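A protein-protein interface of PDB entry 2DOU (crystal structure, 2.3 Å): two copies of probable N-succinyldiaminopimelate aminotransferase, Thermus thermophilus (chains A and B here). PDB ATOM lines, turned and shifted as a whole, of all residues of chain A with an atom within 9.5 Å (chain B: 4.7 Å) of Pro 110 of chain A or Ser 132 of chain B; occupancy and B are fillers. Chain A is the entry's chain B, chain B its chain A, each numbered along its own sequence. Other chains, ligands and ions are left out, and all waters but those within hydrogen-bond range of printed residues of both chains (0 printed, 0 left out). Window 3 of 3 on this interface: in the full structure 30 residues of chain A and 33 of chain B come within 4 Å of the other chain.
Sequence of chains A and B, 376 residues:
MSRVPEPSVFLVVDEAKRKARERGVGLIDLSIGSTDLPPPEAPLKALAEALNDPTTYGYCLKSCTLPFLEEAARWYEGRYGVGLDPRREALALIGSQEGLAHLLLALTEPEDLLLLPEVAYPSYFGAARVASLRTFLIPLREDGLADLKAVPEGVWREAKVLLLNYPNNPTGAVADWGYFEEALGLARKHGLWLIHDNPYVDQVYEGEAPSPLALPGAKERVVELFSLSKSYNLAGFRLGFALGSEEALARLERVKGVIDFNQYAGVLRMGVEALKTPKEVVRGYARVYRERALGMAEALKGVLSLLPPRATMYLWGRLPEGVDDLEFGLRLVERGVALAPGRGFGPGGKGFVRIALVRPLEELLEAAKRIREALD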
ATOM      1  N   LEU A 104       8.843 -18.027 -29.343  1.00  0.00           N
ATOM      2  CA  LEU A 104       9.229 -17.572 -28.014  1.00  0.00           C
ATOM      3  C   LEU A 104       9.791 -18.711 -27.165  1.00  0.00           C
ATOM      4  O   LEU A 104      10.738 -18.518 -26.398  1.00  0.00           O
ATOM      5  CB  LEU A 104       8.048 -16.919 -27.301  1.00  0.00           C
ATOM      6  CG  LEU A 104       7.706 -15.490 -27.725  1.00  0.00           C
ATOM      7  CD1 LEU A 104       6.475 -15.027 -26.963  1.00  0.00           C
ATOM      8  CD2 LEU A 104       8.884 -14.560 -27.444  1.00  0.00           C
ATOM      9  N   LEU A 105       9.208 -19.897 -27.296  1.00  0.00           N
ATOM     10  CA  LEU A 105       9.689 -21.047 -26.547  1.00  0.00           C
ATOM     11  C   LEU A 105      11.050 -21.457 -27.093  1.00  0.00           C
ATOM     12  O   LEU A 105      11.974 -21.750 -26.339  1.00  0.00           O
ATOM     13  CB  LEU A 105       8.711 -22.216 -26.679  1.00  0.00           C
ATOM     14  CG  LEU A 105       7.457 -22.106 -25.807  1.00  0.00           C
ATOM     15  CD1 LEU A 105       6.278 -22.799 -26.487  1.00  0.00           C
ATOM     16  CD2 LEU A 105       7.744 -22.706 -24.429  1.00  0.00           C
ATOM     17  N   ALA A 106      11.152 -21.467 -28.416  1.00  0.00           N
ATOM     18  CA  ALA A 106      12.375 -21.852 -29.095  1.00  0.00           C
ATOM     19  C   ALA A 106      13.596 -21.003 -28.739  1.00  0.00           C
ATOM     20  O   ALA A 106      14.671 -21.545 -28.537  1.00  0.00           O
ATOM     21  CB  ALA A 106      12.152 -21.826 -30.599  1.00  0.00           C
ATOM     22  N   LEU A 107      13.414 -19.690 -28.626  1.00  0.00           N
ATOM     23  CA  LEU A 107      14.524 -18.770 -28.349  1.00  0.00           C
ATOM     24  C   LEU A 107      14.793 -18.388 -26.905  1.00  0.00           C
ATOM     25  O   LEU A 107      15.651 -17.544 -26.649  1.00  0.00           O
ATOM     26  CB  LEU A 107      14.331 -17.471 -29.131  1.00  0.00           C
ATOM     27  CG  LEU A 107      13.909 -17.591 -30.590  1.00  0.00           C
ATOM     28  CD1 LEU A 107      13.780 -16.192 -31.189  1.00  0.00           C
ATOM     29  CD2 LEU A 107      14.905 -18.440 -31.352  1.00  0.00           C
ATOM     30  N   THR A 108      14.082 -18.990 -25.961  1.00  0.00           N
ATOM     31  CA  THR A 108      14.272 -18.625 -24.567  1.00  0.00           C
ATOM     32  C   THR A 108      14.277 -19.776 -23.585  1.00  0.00           C
ATOM     33  O   THR A 108      14.110 -20.939 -23.941  1.00  0.00           O
ATOM     34  CB  THR A 108      13.177 -17.666 -24.102  1.00  0.00           C
ATOM     35  OG1 THR A 108      11.924 -18.365 -24.082  1.00  0.00           O
ATOM     36  CG2 THR A 108      13.075 -16.470 -25.039  1.00  0.00           C
ATOM     37  N   GLU A 109      14.473 -19.407 -22.329  1.00  0.00           N
ATOM     38  CA  GLU A 109      14.491 -20.332 -21.213  1.00  0.00           C
ATOM     39  C   GLU A 109      13.592 -19.663 -20.189  1.00  0.00           C
ATOM     40  O   GLU A 109      13.478 -18.434 -20.168  1.00  0.00           O
ATOM     41  CB  GLU A 109      15.908 -20.464 -20.636  1.00  0.00           C
ATOM     42  CG  GLU A 109      16.915 -21.153 -21.553  1.00  0.00           C
ATOM     43  CD  GLU A 109      16.529 -22.593 -21.842  1.00  0.00           C
ATOM     44  OE1 GLU A 109      16.155 -23.300 -20.877  1.00  0.00           O
ATOM     45  OE2 GLU A 109      16.601 -23.024 -23.023  1.00  0.00           O
ATOM     46  N   PRO A 110      12.931 -20.455 -19.333  1.00  0.00           N
ATOM     47  CA  PRO A 110      12.046 -19.886 -18.312  1.00  0.00           C
ATOM     48  C   PRO A 110      12.723 -18.786 -17.490  1.00  0.00           C
ATOM     49  O   PRO A 110      13.839 -18.954 -17.020  1.00  0.00           O
ATOM     50  CB  PRO A 110      11.677 -21.105 -17.463  1.00  0.00           C
ATOM     51  CG  PRO A 110      11.651 -22.215 -18.481  1.00  0.00           C
ATOM     52  CD  PRO A 110      12.889 -21.930 -19.315  1.00  0.00           C
ATOM     53  N   GLU A 111      12.020 -17.672 -17.331  1.00  0.00           N
ATOM     54  CA  GLU A 111      12.466 -16.507 -16.572  1.00  0.00           C
ATOM     55  C   GLU A 111      13.280 -15.488 -17.359  1.00  0.00           C
ATOM     56  O   GLU A 111      13.681 -14.462 -16.806  1.00  0.00           O
ATOM     57  CB  GLU A 111      13.225 -16.916 -15.298  1.00  0.00           C
ATOM     58  CG  GLU A 111      12.353 -17.642 -14.256  1.00  0.00           C
ATOM     59  CD  GLU A 111      10.997 -16.964 -14.044  1.00  0.00           C
ATOM     60  OE1 GLU A 111      10.954 -15.813 -13.549  1.00  0.00           O
ATOM     61  OE2 GLU A 111       9.964 -17.579 -14.387  1.00  0.00           O
ATOM     62  N   ASP A 112      13.533 -15.768 -18.640  1.00  0.00           N
ATOM     63  CA  ASP A 112      14.250 -14.822 -19.492  1.00  0.00           C
ATOM     64  C   ASP A 112      13.321 -13.630 -19.624  1.00  0.00           C
ATOM     65  O   ASP A 112      12.107 -13.780 -19.475  1.00  0.00           O
ATOM     66  CB  ASP A 112      14.506 -15.412 -20.880  1.00  0.00           C
ATOM     67  CG  ASP A 112      15.696 -16.339 -20.907  1.00  0.00           C
ATOM     68  OD1 ASP A 112      16.397 -16.435 -19.880  1.00  0.00           O
ATOM     69  OD2 ASP A 112      15.937 -16.963 -21.958  1.00  0.00           O
ATOM     70  N   LEU A 113      13.869 -12.454 -19.910  1.00  0.00           N
ATOM     71  CA  LEU A 113      13.046 -11.256 -20.029  1.00  0.00           C
ATOM     72  C   LEU A 113      12.673 -10.906 -21.460  1.00  0.00           C
ATOM     73  O   LEU A 113      13.529 -10.888 -22.350  1.00  0.00           O
ATOM     74  CB  LEU A 113      13.755 -10.060 -19.390  1.00  0.00           C
ATOM     75  CG  LEU A 113      13.049  -8.708 -19.519  1.00  0.00           C
ATOM     76  CD1 LEU A 113      11.688  -8.770 -18.818  1.00  0.00           C
ATOM     77  CD2 LEU A 113      13.907  -7.616 -18.913  1.00  0.00           C
ATOM     78  N   LEU A 114      11.386 -10.626 -21.670  1.00  0.00           N
ATOM     79  CA  LEU A 114      10.868 -10.255 -22.980  1.00  0.00           C
ATOM     80  C   LEU A 114      10.437  -8.806 -22.938  1.00  0.00           C
ATOM     81  O   LEU A 114       9.934  -8.331 -21.921  1.00  0.00           O
ATOM     82  CB  LEU A 114       9.662 -11.116 -23.356  1.00  0.00           C
ATOM     83  CG  LEU A 114       8.804 -10.597 -24.518  1.00  0.00           C
ATOM     84  CD1 LEU A 114       9.626 -10.543 -25.807  1.00  0.00           C
ATOM     85  CD2 LEU A 114       7.591 -11.502 -24.689  1.00  0.00           C
ATOM     86  N   ALA A 128       3.751 -15.149 -23.844  1.00  0.00           N
ATOM     87  CA  ALA A 128       4.804 -14.836 -22.889  1.00  0.00           C
ATOM     88  C   ALA A 128       4.649 -15.694 -21.629  1.00  0.00           C
ATOM     89  O   ALA A 128       5.627 -16.258 -21.131  1.00  0.00           O
ATOM     90  CB  ALA A 128       4.754 -13.366 -22.528  1.00  0.00           C
ATOM     91  N   ARG A 129       3.423 -15.797 -21.112  1.00  0.00           N
ATOM     92  CA  ARG A 129       3.190 -16.609 -19.917  1.00  0.00           C
ATOM     93  C   ARG A 129       3.403 -18.090 -20.226  1.00  0.00           C
ATOM     94  O   ARG A 129       3.915 -18.829 -19.398  1.00  0.00           O
ATOM     95  CB  ARG A 129       1.776 -16.374 -19.373  1.00  0.00           C
ATOM     96  N   VAL A 130       3.030 -18.518 -21.428  1.00  0.00           N
ATOM     97  CA  VAL A 130       3.199 -19.916 -21.820  1.00  0.00           C
ATOM     98  C   VAL A 130       4.669 -20.328 -21.807  1.00  0.00           C
ATOM     99  O   VAL A 130       5.004 -21.472 -21.491  1.00  0.00           O
ATOM    100  CB  VAL A 130       2.643 -20.173 -23.237  1.00  0.00           C
ATOM    101  CG1 VAL A 130       2.907 -21.607 -23.659  1.00  0.00           C
ATOM    102  CG2 VAL A 130       1.162 -19.881 -23.267  1.00  0.00           C
ATOM    103  N   ALA A 131       5.547 -19.392 -22.160  1.00  0.00           N
ATOM    104  CA  ALA A 131       6.975 -19.678 -22.191  1.00  0.00           C
ATOM    105  C   ALA A 131       7.613 -19.356 -20.847  1.00  0.00           C
ATOM    106  O   ALA A 131       8.830 -19.371 -20.720  1.00  0.00           O
ATOM    107  CB  ALA A 131       7.647 -18.872 -23.307  1.00  0.00           C
ATOM    108  N   SER A 132       6.779 -19.068 -19.847  1.00  0.00           N
ATOM    109  CA  SER A 132       7.243 -18.738 -18.497  1.00  0.00           C
ATOM    110  C   SER A 132       8.231 -17.581 -18.534  1.00  0.00           C
ATOM    111  O   SER A 132       9.254 -17.619 -17.865  1.00  0.00           O
ATOM    112  CB  SER A 132       7.926 -19.949 -17.843  1.00  0.00           C
ATOM    113  OG  SER A 132       7.058 -21.060 -17.738  1.00  0.00           O
ATOM    114  N   LEU A 133       7.918 -16.542 -19.297  1.00  0.00           N
ATOM    115  CA  LEU A 133       8.826 -15.408 -19.408  1.00  0.00           C
ATOM    116  C   LEU A 133       8.446 -14.197 -18.584  1.00  0.00           C
ATOM    117  O   LEU A 133       7.270 -13.905 -18.389  1.00  0.00           O
ATOM    118  CB  LEU A 133       8.940 -14.965 -20.868  1.00  0.00           C
ATOM    119  CG  LEU A 133       9.416 -16.010 -21.874  1.00  0.00           C
ATOM    120  CD1 LEU A 133       9.388 -15.415 -23.265  1.00  0.00           C
ATOM    121  CD2 LEU A 133      10.811 -16.490 -21.505  1.00  0.00           C
ATOM    122  N   ARG A 134       9.457 -13.485 -18.102  1.00  0.00           N
ATOM    123  CA  ARG A 134       9.218 -12.259 -17.361  1.00  0.00           C
ATOM    124  C   ARG A 134       9.025 -11.247 -18.477  1.00  0.00           C
ATOM    125  O   ARG A 134       9.485 -11.469 -19.601  1.00  0.00           O
ATOM    126  CB  ARG A 134      10.434 -11.890 -16.521  1.00  0.00           C
ATOM    127  CG  ARG A 134      10.684 -12.829 -15.356  1.00  0.00           C
ATOM    128  CD  ARG A 134      12.103 -12.668 -14.868  1.00  0.00           C
ATOM    129  NE  ARG A 134      12.428 -11.263 -14.668  1.00  0.00           N
ATOM    130  CZ  ARG A 134      13.598 -10.712 -14.981  1.00  0.00           C
ATOM    131  NH1 ARG A 134      14.560 -11.454 -15.516  1.00  0.00           N
ATOM    132  NH2 ARG A 134      13.803  -9.418 -14.755  1.00  0.00           N
ATOM    133  N   LYS A 160      16.207 -10.403 -23.565  1.00  0.00           N
ATOM    134  CA  LYS A 160      16.700 -11.468 -24.423  1.00  0.00           C
ATOM    135  C   LYS A 160      15.938 -11.422 -25.742  1.00  0.00           C
ATOM    136  O   LYS A 160      16.427 -11.882 -26.774  1.00  0.00           O
ATOM    137  CB  LYS A 160      16.511 -12.819 -23.749  1.00  0.00           C
ATOM    138  N   PRO B 110       7.841 -25.388 -15.207  1.00  0.00           N
ATOM    139  CA  PRO B 110       9.209 -25.826 -15.469  1.00  0.00           C
ATOM    140  C   PRO B 110       9.759 -26.594 -14.270  1.00  0.00           C
ATOM    141  O   PRO B 110       9.547 -26.203 -13.118  1.00  0.00           O
ATOM    142  CB  PRO B 110       9.936 -24.510 -15.717  1.00  0.00           C
ATOM    143  CG  PRO B 110       8.901 -23.742 -16.484  1.00  0.00           C
ATOM    144  CD  PRO B 110       7.637 -24.003 -15.673  1.00  0.00           C
ATOM    145  N   GLU B 111      10.440 -27.697 -14.562  1.00  0.00           N
ATOM    146  CA  GLU B 111      11.041 -28.570 -13.562  1.00  0.00           C
ATOM    147  C   GLU B 111      10.069 -29.566 -12.908  1.00  0.00           C
ATOM    148  O   GLU B 111      10.470 -30.325 -12.031  1.00  0.00           O
ATOM    149  CB  GLU B 111      11.765 -27.751 -12.483  1.00  0.00           C
ATOM    150  CG  GLU B 111      12.867 -26.826 -13.019  1.00  0.00           C
ATOM    151  CD  GLU B 111      13.906 -27.556 -13.874  1.00  0.00           C
ATOM    152  OE1 GLU B 111      14.609 -28.452 -13.346  1.00  0.00           O
ATOM    153  OE2 GLU B 111      14.020 -27.236 -15.083  1.00  0.00           O
ATOM    154  N   ASP B 112       8.800 -29.569 -13.312  1.00  0.00           N
ATOM    155  CA  ASP B 112       7.866 -30.546 -12.749  1.00  0.00           C
ATOM    156  C   ASP B 112       8.329 -31.888 -13.303  1.00  0.00           C
ATOM    157  O   ASP B 112       8.953 -31.932 -14.360  1.00  0.00           O
ATOM    158  CB  ASP B 112       6.420 -30.291 -13.197  1.00  0.00           C
ATOM    159  CG  ASP B 112       5.733 -29.205 -12.391  1.00  0.00           C
ATOM    160  OD1 ASP B 112       6.184 -28.904 -11.266  1.00  0.00           O
ATOM    161  OD2 ASP B 112       4.724 -28.660 -12.880  1.00  0.00           O
ATOM    162  N   ALA B 128       8.360 -32.973 -23.694  1.00  0.00           N
ATOM    163  CA  ALA B 128       8.737 -32.791 -22.302  1.00  0.00           C
ATOM    164  C   ALA B 128       9.794 -31.691 -22.196  1.00  0.00           C
ATOM    165  O   ALA B 128       9.751 -30.862 -21.283  1.00  0.00           O
ATOM    166  CB  ALA B 128       9.276 -34.091 -21.731  1.00  0.00           C
ATOM    167  N   ARG B 129      10.748 -31.680 -23.130  1.00  0.00           N
ATOM    168  CA  ARG B 129      11.791 -30.653 -23.106  1.00  0.00           C
ATOM    169  C   ARG B 129      11.199 -29.273 -23.347  1.00  0.00           C
ATOM    170  O   ARG B 129      11.569 -28.307 -22.688  1.00  0.00           O
ATOM    171  CB  ARG B 129      12.870 -30.916 -24.159  1.00  0.00           C
ATOM    172  CG  ARG B 129      13.900 -29.772 -24.248  1.00  0.00           C
ATOM    173  CD  ARG B 129      15.330 -30.288 -24.159  1.00  0.00           C
ATOM    174  NE  ARG B 129      15.828 -30.764 -25.450  1.00  0.00           N
ATOM    175  CZ  ARG B 129      16.724 -31.742 -25.585  1.00  0.00           C
ATOM    176  NH1 ARG B 129      17.212 -32.354 -24.501  1.00  0.00           N
ATOM    177  NH2 ARG B 129      17.146 -32.100 -26.801  1.00  0.00           N
ATOM    178  N   VAL B 130      10.282 -29.177 -24.299  1.00  0.00           N
ATOM    179  CA  VAL B 130       9.660 -27.895 -24.595  1.00  0.00           C
ATOM    180  C   VAL B 130       8.992 -27.331 -23.348  1.00  0.00           C
ATOM    181  O   VAL B 130       8.944 -26.116 -23.147  1.00  0.00           O
ATOM    182  CB  VAL B 130       8.615 -28.035 -25.707  1.00  0.00           C
ATOM    183  CG1 VAL B 130       7.988 -26.688 -25.995  1.00  0.00           C
ATOM    184  CG2 VAL B 130       9.266 -28.605 -26.962  1.00  0.00           C
ATOM    185  N   ALA B 131       8.490 -28.227 -22.502  1.00  0.00           N
ATOM    186  CA  ALA B 131       7.815 -27.844 -21.265  1.00  0.00           C
ATOM    187  C   ALA B 131       8.794 -27.634 -20.111  1.00  0.00           C
ATOM    188  O   ALA B 131       8.382 -27.263 -19.005  1.00  0.00           O
ATOM    189  CB  ALA B 131       6.783 -28.913 -20.885  1.00  0.00           C
ATOM    190  N   SER B 132      10.082 -27.872 -20.372  1.00  0.00           N
ATOM    191  CA  SER B 132      11.135 -27.708 -19.364  1.00  0.00           C
ATOM    192  C   SER B 132      10.882 -28.673 -18.224  1.00  0.00           C
ATOM    193  O   SER B 132      11.093 -28.347 -17.056  1.00  0.00           O
ATOM    194  CB  SER B 132      11.143 -26.283 -18.808  1.00  0.00           C
ATOM    195  OG  SER B 132      11.300 -25.330 -19.836  1.00  0.00           O
ATOM    196  N   LEU B 133      10.436 -29.868 -18.572  1.00  0.00           N
ATOM    197  CA  LEU B 133      10.117 -30.869 -17.571  1.00  0.00           C
ATOM    198  C   LEU B 133      11.223 -31.881 -17.354  1.00  0.00           C
ATOM    199  O   LEU B 133      11.964 -32.218 -18.275  1.00  0.00           O
ATOM    200  CB  LEU B 133       8.849 -31.619 -17.976  1.00  0.00           C
ATOM    201  CG  LEU B 133       7.552 -30.842 -18.183  1.00  0.00           C
ATOM    202  CD1 LEU B 133       6.463 -31.815 -18.645  1.00  0.00           C
ATOM    203  CD2 LEU B 133       7.151 -30.140 -16.891  1.00  0.00           C
ATOM    204  N   ARG B 134      11.326 -32.360 -16.121  1.00  0.00           N
ATOM    205  CA  ARG B 134      12.297 -33.383 -15.780  1.00  0.00           C
ATOM    206  C   ARG B 134      11.553 -34.682 -16.058  1.00  0.00           C
ATOM    207  O   ARG B 134      10.323 -34.694 -16.112  1.00  0.00           O
ATOM    208  CB  ARG B 134      12.664 -33.292 -14.299  1.00  0.00           C
ATOM    209  CG  ARG B 134      13.405 -32.020 -13.942  1.00  0.00           C
ATOM    210  CD  ARG B 134      13.066 -31.580 -12.533  1.00  0.00           C
ATOM    211  NE  ARG B 134      13.341 -32.616 -11.551  1.00  0.00           N
ATOM    212  CZ  ARG B 134      12.493 -32.967 -10.585  1.00  0.00           C
ATOM    213  NH1 ARG B 134      11.310 -32.362 -10.477  1.00  0.00           N
ATOM    214  NH2 ARG B 134      12.829 -33.917  -9.717  1.00  0.00           N
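The backbone NH (N) of Glu 111 of chain A sits at hydrogen-bond distance from the backbone carbonyl oxygen (O) of Ser 132 of chain A (2.8 Å).
N of Glu 111 of chain B sits at hydrogen-bond distance from O of Ser 132 of chain B, 2.7 Å away.
Leu 105 of chain A touches Val 130 of chain B (CD2 to O, 3.8 Å).
CG of Pro 110 of chain A touches CG of Pro 110 of chain B (3.7 Å).
OG of Ser 132 of chain B touches CG of Pro 110 of chain A, 3.4 Å away.
CG of Pro 110 of chain B touches OG of Ser 132 of chain A (3.5 Å).
Printed residues of chain B within 4 Å of Leu 105 of chain A: Val 130 (3.8 Å).
Asp 112 of chain A touches none of the printed residues of chain B.
Printed residues of chain B within 4 Å of Ser 132 of chain A: Pro 110 (3.5 Å).
Of the printed residues of chain A, Val 130 of chain B touches Leu 105.
No residue of chain A comes within 4 Å of Ala 131 of chain B.
Of chain A, only Pro 110 (3.4 Å) comes within 4 Å of Ser 132 of chain B.
No residue of chain A comes within 4 Å of Leu 133 of chain B.
Arg 134 of chain B touches none of the printed residues of chain A.
The nearest residue of chain A that does not touch Ser 132 of chain B is Glu 109 of chain A (5.4 Å).
Of the 10 printed residues of chain B, 3 touch a printed residue of chain A.
Hydrophobic or aromatic side chains of chain B that line the printed part of chain A: Pro 110.
Of the 19 printed residues of chain A, 3 touch a printed residue of chain B.
Along chain A the printed residues that touch a printed residue of chain B span positions 105 to 132.
Among the printed residues, 4 pairs touch across the chains.
Among the printed residues, no Asp or Glu carboxylate lies within 4 Å of a Lys or Arg side-chain nitrogen of the other chain.
Pro 110 of chain A touches its own counterpart, Pro 110 of chain B.
Pro 110 of chain A touches Ser 132 of chain B, and with the chains exchanged Ser 132 of chain A touches Pro 110 of chain B.
10 positions are printed for both chains.
Of the 4 pairs that touch across the chains among the printed residues, 3 have their exchanged pair printed and touching as well.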
